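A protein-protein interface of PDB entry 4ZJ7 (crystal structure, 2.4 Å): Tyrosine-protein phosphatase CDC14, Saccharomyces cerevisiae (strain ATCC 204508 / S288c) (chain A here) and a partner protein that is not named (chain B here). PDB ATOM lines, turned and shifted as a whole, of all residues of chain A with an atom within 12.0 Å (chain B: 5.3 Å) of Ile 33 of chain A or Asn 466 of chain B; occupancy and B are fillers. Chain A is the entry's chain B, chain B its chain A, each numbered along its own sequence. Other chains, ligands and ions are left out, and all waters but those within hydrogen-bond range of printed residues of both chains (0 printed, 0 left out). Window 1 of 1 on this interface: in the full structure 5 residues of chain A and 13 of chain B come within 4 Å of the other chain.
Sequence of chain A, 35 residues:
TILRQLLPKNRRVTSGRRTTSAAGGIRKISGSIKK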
ATOM      1  N   GLY A  31      -1.450  -4.620  12.126  1.00  0.00           N
ATOM      2  CA  GLY A  31      -1.950  -3.545  11.290  1.00  0.00           C
ATOM      3  C   GLY A  31      -1.816  -3.841   9.809  1.00  0.00           C
ATOM      4  O   GLY A  31      -1.382  -2.990   9.034  1.00  0.00           O
ATOM      5  N   SER A  32      -2.185  -5.056   9.418  1.00  0.00           N
ATOM      6  CA  SER A  32      -2.178  -5.447   8.013  1.00  0.00           C
ATOM      7  C   SER A  32      -3.539  -6.011   7.620  1.00  0.00           C
ATOM      8  O   SER A  32      -4.428  -6.146   8.459  1.00  0.00           O
ATOM      9  CB  SER A  32      -1.076  -6.474   7.739  1.00  0.00           C
ATOM     10  OG  SER A  32      -1.302  -7.673   8.462  1.00  0.00           O
ATOM     11  N   ILE A  33      -3.701  -6.332   6.342  1.00  0.00           N
ATOM     12  CA  ILE A  33      -4.950  -6.908   5.861  1.00  0.00           C
ATOM     13  C   ILE A  33      -4.813  -8.417   5.699  1.00  0.00           C
ATOM     14  O   ILE A  33      -3.933  -8.900   4.986  1.00  0.00           O
ATOM     15  CB  ILE A  33      -5.387  -6.272   4.529  1.00  0.00           C
ATOM     16  CG1 ILE A  33      -5.877  -4.843   4.773  1.00  0.00           C
ATOM     17  CG2 ILE A  33      -6.484  -7.099   3.871  1.00  0.00           C
ATOM     18  CD1 ILE A  33      -6.186  -4.078   3.514  1.00  0.00           C
ATOM     19  N   LYS A  34      -5.685  -9.159   6.375  1.00  0.00           N
ATOM     20  CA  LYS A  34      -5.617 -10.614   6.364  1.00  0.00           C
ATOM     21  C   LYS A  34      -6.999 -11.250   6.456  1.00  0.00           C
ATOM     22  O   LYS A  34      -7.956 -10.623   6.911  1.00  0.00           O
ATOM     23  CB  LYS A  34      -4.739 -11.112   7.513  1.00  0.00           C
ATOM     24  N   LYS A  35      -7.094 -12.500   6.016  1.00  0.00           N
ATOM     25  CA  LYS A  35      -8.334 -13.257   6.113  1.00  0.00           C
ATOM     26  C   LYS A  35      -8.446 -13.910   7.486  1.00  0.00           C
ATOM     27  O   LYS A  35      -7.438 -14.199   8.131  1.00  0.00           O
ATOM     28  CB  LYS A  35      -8.407 -14.315   5.010  1.00  0.00           C
ATOM     29  CG  LYS A  35      -8.319 -13.747   3.602  1.00  0.00           C
ATOM     30  CD  LYS A  35      -8.281 -14.850   2.556  1.00  0.00           C
ATOM     31  CE  LYS A  35      -6.984 -15.637   2.632  1.00  0.00           C
ATOM     32  NZ  LYS A  35      -6.886 -16.650   1.546  1.00  0.00           N
ATOM     33  OXT LYS A  35      -9.542 -14.163   7.986  1.00  0.00           O
ATOM     34  N   CYS B 418      -9.866  -0.994  -0.852  1.00  0.00           N
ATOM     35  CA  CYS B 418      -8.550  -0.990  -0.223  1.00  0.00           C
ATOM     36  C   CYS B 418      -8.179  -2.390   0.249  1.00  0.00           C
ATOM     37  O   CYS B 418      -7.017  -2.793   0.185  1.00  0.00           O
ATOM     38  CB  CYS B 418      -8.510  -0.017   0.959  1.00  0.00           C
ATOM     39  SG  CYS B 418      -8.668   1.727   0.515  1.00  0.00           S
ATOM     40  N   ASN B 419      -9.182  -3.122   0.718  1.00  0.00           N
ATOM     41  CA  ASN B 419      -8.983  -4.466   1.245  1.00  0.00           C
ATOM     42  C   ASN B 419      -8.500  -5.438   0.174  1.00  0.00           C
ATOM     43  O   ASN B 419      -7.656  -6.293   0.443  1.00  0.00           O
ATOM     44  CB  ASN B 419     -10.279  -4.976   1.876  1.00  0.00           C
ATOM     45  CG  ASN B 419     -10.100  -6.296   2.606  1.00  0.00           C
ATOM     46  OD1 ASN B 419      -9.958  -7.349   1.987  1.00  0.00           O
ATOM     47  ND2 ASN B 419     -10.123  -6.244   3.932  1.00  0.00           N
ATOM     48  N   GLY B 422      -4.902  -4.703  -0.784  1.00  0.00           N
ATOM     49  CA  GLY B 422      -4.087  -5.210   0.301  1.00  0.00           C
ATOM     50  C   GLY B 422      -3.936  -6.717   0.221  1.00  0.00           C
ATOM     51  O   GLY B 422      -2.822  -7.238   0.221  1.00  0.00           O
ATOM     52  N   GLN B 423      -5.063  -7.417   0.137  1.00  0.00           N
ATOM     53  CA  GLN B 423      -5.060  -8.877   0.124  1.00  0.00           C
ATOM     54  C   GLN B 423      -4.296  -9.446  -1.070  1.00  0.00           C
ATOM     55  O   GLN B 423      -3.532 -10.401  -0.927  1.00  0.00           O
ATOM     56  CB  GLN B 423      -6.492  -9.413   0.124  1.00  0.00           C
ATOM     57  CG  GLN B 423      -6.579 -10.925   0.234  1.00  0.00           C
ATOM     58  CD  GLN B 423      -6.037 -11.449   1.551  1.00  0.00           C
ATOM     59  OE1 GLN B 423      -6.467 -11.025   2.624  1.00  0.00           O
ATOM     60  NE2 GLN B 423      -5.087 -12.374   1.475  1.00  0.00           N
ATOM     61  N   SER B 425      -1.995  -7.943  -2.779  1.00  0.00           N
ATOM     62  CA  SER B 425      -0.586  -7.572  -2.687  1.00  0.00           C
ATOM     63  C   SER B 425       0.196  -8.682  -1.993  1.00  0.00           C
ATOM     64  O   SER B 425       1.388  -8.864  -2.235  1.00  0.00           O
ATOM     65  CB  SER B 425      -0.410  -6.250  -1.935  1.00  0.00           C
ATOM     66  OG  SER B 425      -0.926  -5.161  -2.681  1.00  0.00           O
ATOM     67  N   THR B 426      -0.492  -9.421  -1.129  1.00  0.00           N
ATOM     68  CA  THR B 426       0.096 -10.569  -0.451  1.00  0.00           C
ATOM     69  C   THR B 426       0.002 -11.824  -1.312  1.00  0.00           C
ATOM     70  O   THR B 426       1.004 -12.490  -1.572  1.00  0.00           O
ATOM     71  CB  THR B 426      -0.594 -10.840   0.900  1.00  0.00           C
ATOM     72  OG1 THR B 426      -0.346  -9.751   1.796  1.00  0.00           O
ATOM     73  CG2 THR B 426      -0.069 -12.128   1.518  1.00  0.00           C
ATOM     74  N   GLN B 433       4.010  -6.564  -7.009  1.00  0.00           N
ATOM     75  CA  GLN B 433       4.790  -5.411  -6.568  1.00  0.00           C
ATOM     76  C   GLN B 433       5.627  -4.855  -7.717  1.00  0.00           C
ATOM     77  O   GLN B 433       5.722  -3.642  -7.900  1.00  0.00           O
ATOM     78  CB  GLN B 433       5.701  -5.780  -5.392  1.00  0.00           C
ATOM     79  CG  GLN B 433       5.008  -5.832  -4.036  1.00  0.00           C
ATOM     80  CD  GLN B 433       4.211  -7.104  -3.826  1.00  0.00           C
ATOM     81  OE1 GLN B 433       4.290  -8.040  -4.621  1.00  0.00           O
ATOM     82  NE2 GLN B 433       3.441  -7.146  -2.744  1.00  0.00           N
ATOM     83  N   HIS B 459      -7.573   1.707   6.536  1.00  0.00           N
ATOM     84  CA  HIS B 459      -7.533   0.465   5.774  1.00  0.00           C
ATOM     85  C   HIS B 459      -6.599   0.576   4.576  1.00  0.00           C
ATOM     86  O   HIS B 459      -5.979  -0.408   4.171  1.00  0.00           O
ATOM     87  CB  HIS B 459      -8.934   0.069   5.315  1.00  0.00           C
ATOM     88  CG  HIS B 459      -9.158  -1.410   5.285  1.00  0.00           C
ATOM     89  ND1 HIS B 459      -8.971  -2.210   6.393  1.00  0.00           N
ATOM     90  CD2 HIS B 459      -9.553  -2.236   4.289  1.00  0.00           C
ATOM     91  CE1 HIS B 459      -9.241  -3.463   6.080  1.00  0.00           C
ATOM     92  NE2 HIS B 459      -9.597  -3.507   4.807  1.00  0.00           N
ATOM     93  N   ALA B 462      -3.311   0.201   6.048  1.00  0.00           N
ATOM     94  CA  ALA B 462      -3.133  -1.214   6.346  1.00  0.00           C
ATOM     95  C   ALA B 462      -2.730  -1.980   5.092  1.00  0.00           C
ATOM     96  O   ALA B 462      -1.871  -2.859   5.139  1.00  0.00           O
ATOM     97  CB  ALA B 462      -4.405  -1.798   6.942  1.00  0.00           C
ATOM     98  N   ALA B 463      -3.356  -1.635   3.970  1.00  0.00           N
ATOM     99  CA  ALA B 463      -3.059  -2.269   2.691  1.00  0.00           C
ATOM    100  C   ALA B 463      -1.628  -1.980   2.247  1.00  0.00           C
ATOM    101  O   ALA B 463      -1.019  -2.773   1.529  1.00  0.00           O
ATOM    102  CB  ALA B 463      -4.044  -1.805   1.628  1.00  0.00           C
ATOM    103  N   LEU B 464      -1.098  -0.841   2.680  1.00  0.00           N
ATOM    104  CA  LEU B 464       0.269  -0.453   2.345  1.00  0.00           C
ATOM    105  C   LEU B 464       1.287  -1.353   3.039  1.00  0.00           C
ATOM    106  O   LEU B 464       2.411  -1.506   2.566  1.00  0.00           O
ATOM    107  CB  LEU B 464       0.516   1.011   2.715  1.00  0.00           C
ATOM    108  CG  LEU B 464      -0.123   2.041   1.781  1.00  0.00           C
ATOM    109  CD1 LEU B 464      -0.056   3.436   2.381  1.00  0.00           C
ATOM    110  CD2 LEU B 464       0.549   2.012   0.419  1.00  0.00           C
ATOM    111  N   VAL B 465       0.889  -1.945   4.161  1.00  0.00           N
ATOM    112  CA  VAL B 465       1.737  -2.905   4.860  1.00  0.00           C
ATOM    113  C   VAL B 465       1.869  -4.187   4.044  1.00  0.00           C
ATOM    114  O   VAL B 465       2.965  -4.728   3.889  1.00  0.00           O
ATOM    115  CB  VAL B 465       1.184  -3.244   6.259  1.00  0.00           C
ATOM    116  CG1 VAL B 465       2.048  -4.303   6.932  1.00  0.00           C
ATOM    117  CG2 VAL B 465       1.103  -1.993   7.114  1.00  0.00           C
ATOM    118  N   ASN B 466       0.742  -4.665   3.525  1.00  0.00           N
ATOM    119  CA  ASN B 466       0.721  -5.852   2.678  1.00  0.00           C
ATOM    120  C   ASN B 466       1.595  -5.687   1.440  1.00  0.00           C
ATOM    121  O   ASN B 466       2.357  -6.584   1.080  1.00  0.00           O
ATOM    122  CB  ASN B 466      -0.711  -6.179   2.250  1.00  0.00           C
ATOM    123  CG  ASN B 466      -1.596  -6.573   3.416  1.00  0.00           C
ATOM    124  OD1 ASN B 466      -2.012  -5.728   4.209  1.00  0.00           O
ATOM    125  ND2 ASN B 466      -1.902  -7.861   3.517  1.00  0.00           N
ATOM    126  N   PHE B 467       1.477  -4.532   0.792  1.00  0.00           N
ATOM    127  CA  PHE B 467       2.239  -4.250  -0.418  1.00  0.00           C
ATOM    128  C   PHE B 467       3.730  -4.135  -0.118  1.00  0.00           C
ATOM    129  O   PHE B 467       4.563  -4.657  -0.860  1.00  0.00           O
ATOM    130  CB  PHE B 467       1.734  -2.964  -1.081  1.00  0.00           C
ATOM    131  CG  PHE B 467       2.338  -2.697  -2.433  1.00  0.00           C
ATOM    132  CD1 PHE B 467       1.706  -3.133  -3.586  1.00  0.00           C
ATOM    133  CD2 PHE B 467       3.533  -2.005  -2.551  1.00  0.00           C
ATOM    134  CE1 PHE B 467       2.257  -2.890  -4.830  1.00  0.00           C
ATOM    135  CE2 PHE B 467       4.089  -1.760  -3.792  1.00  0.00           C
ATOM    136  CZ  PHE B 467       3.449  -2.202  -4.933  1.00  0.00           C
ATOM    137  N   SER B 468       4.058  -3.453   0.975  1.00  0.00           N
ATOM    138  CA  SER B 468       5.448  -3.169   1.324  1.00  0.00           C
ATOM    139  C   SER B 468       6.246  -4.424   1.662  1.00  0.00           C
ATOM    140  O   SER B 468       7.458  -4.463   1.453  1.00  0.00           O
ATOM    141  CB  SER B 468       5.510  -2.197   2.506  1.00  0.00           C
ATOM    142  OG  SER B 468       5.085  -0.900   2.124  1.00  0.00           O
ATOM    143  N   GLU B 469       5.564  -5.443   2.177  1.00  0.00           N
ATOM    144  CA  GLU B 469       6.229  -6.648   2.672  1.00  0.00           C
ATOM    145  C   GLU B 469       7.097  -7.330   1.617  1.00  0.00           C
ATOM    146  O   GLU B 469       8.121  -7.930   1.942  1.00  0.00           O
ATOM    147  CB  GLU B 469       5.196  -7.644   3.207  1.00  0.00           C
ATOM    148  CG  GLU B 469       5.809  -8.814   3.967  1.00  0.00           C
ATOM    149  CD  GLU B 469       4.782  -9.839   4.404  1.00  0.00           C
ATOM    150  OE1 GLU B 469       5.186 -10.944   4.822  1.00  0.00           O
ATOM    151  OE2 GLU B 469       3.572  -9.540   4.332  1.00  0.00           O
ATOM    152  N   PHE B 470       6.694  -7.232   0.354  1.00  0.00           N
ATOM    153  CA  PHE B 470       7.422  -7.896  -0.721  1.00  0.00           C
ATOM    154  C   PHE B 470       7.859  -6.929  -1.818  1.00  0.00           C
ATOM    155  O   PHE B 470       8.162  -7.342  -2.936  1.00  0.00           O
ATOM    156  CB  PHE B 470       6.570  -9.015  -1.320  1.00  0.00           C
ATOM    157  CG  PHE B 470       6.267 -10.125  -0.354  1.00  0.00           C
ATOM    158  CD1 PHE B 470       7.236 -11.062  -0.032  1.00  0.00           C
ATOM    159  CD2 PHE B 470       5.018 -10.230   0.234  1.00  0.00           C
ATOM    160  CE1 PHE B 470       6.964 -12.083   0.857  1.00  0.00           C
ATOM    161  CE2 PHE B 470       4.740 -11.250   1.124  1.00  0.00           C
ATOM    162  CZ  PHE B 470       5.714 -12.178   1.436  1.00  0.00           C
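Printed residues of chain A that touch a printed residue of chain B: Gly 31, Ser 32, Ile 33, Lys 34 and Lys 35. Hydrophobic or aromatic side chains of chain A that line the printed part of chain B: Ile 33. Along chain A the printed residues that touch a printed residue of chain B span positions 31 to 35. Along chain B the printed residues that touch a printed residue of chain A span positions 418 to 466. Among the printed residues, 12 pairs touch across the chains.
Printed residues of chain B within 4 Å of Gly 31 of chain A: Ala 462 and Val 465. Of the printed residues of chain B, Ile 33 of chain A touches Cys 418 (3.7 Å), Asn 419 (3.6 Å), His 459 (3.7 Å), Ala 463 (3.6 Å) and Asn 466 (2.7 Å). Of the printed residues of chain B, Lys 34 of chain A touches Gln 423 (3.9 Å). Printed residues of chain B within 4 Å of Lys 35 of chain A: Gln 423. Cys 418 of chain B touches one residue of chain A. Printed residues of chain A within 4 Å of Gln 423 of chain B: Lys 34 (3.9 Å) and Lys 35 (3.4 Å). His 459 of chain B touches one residue of chain A. Ala 463 of chain B touches just one residue of chain A: Ile 33. Leu 464 of chain B touches none of the printed residues of chain A. Val 465 of chain B touches just these residues of chain A: Gly 31 and Ser 32. Asn 466 of chain B touches just these residues of chain A: Ser 32 (3.7 Å) and Ile 33 (2.7 Å). Phe 467 of chain B touches none of the printed residues of chain A. No residue of chain A comes within 4 Å of Ser 468 of chain B. No residue of chain A comes within 4 Å of Glu 469 of chain B. The nearest residue of chain A that does not touch Asn 466 of chain B is Lys 34 of chain A (4.9 Å).
The side-chain amide nitrogen (ND2) of Asn 466 of chain B is in hydrogen-bond range of the backbone carbonyl oxygen (O) of Ile 33 of chain A (2.7 Å).
The side-chain amide nitrogen (ND2) of Asn 419 of chain B sits at hydrogen-bond distance from a ring nitrogen (NE2) of His 459 of chain B (2.9 Å). The backbone carbonyl oxygen (O) of Gly 422 of chain B lies close to the side-chain amide nitrogen (ND2) of Asn 466 of chain B (3.5 Å). The backbone carbonyl oxygen (O) of Ala 462 of chain B lies close to the side-chain amide oxygen (OD1) of Asn 466 of chain B (3.0 Å). The side-chain amide nitrogen (ND2) of Asn 466 of chain B sits at hydrogen-bond distance from the side-chain hydroxyl (OG1) of Thr 426 of chain B (3.0 Å).
Among the printed residues, merely in contact across the chains: Gly 31 of chain A with Val 465 of chain B, Lys 35 of chain A with Gln 423 of chain B, Ile 33 of chain A with Asn 419 of chain B, Ile 33 of chain A with Ala 463 of chain B, Ile 33 of chain A with Cys 418 of chain B, Gly 31 of chain A with Ala 462 of chain B, Ile 33 of chain A with His 459 of chain B, Ser 32 of chain A with Asn 466 of chain B, Lys 34 of chain A with Gln 423 of chain B, Ser 32 of chain A with Ala 462 of chain B and Ser 32 of chain A with Val 465 of chain B.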
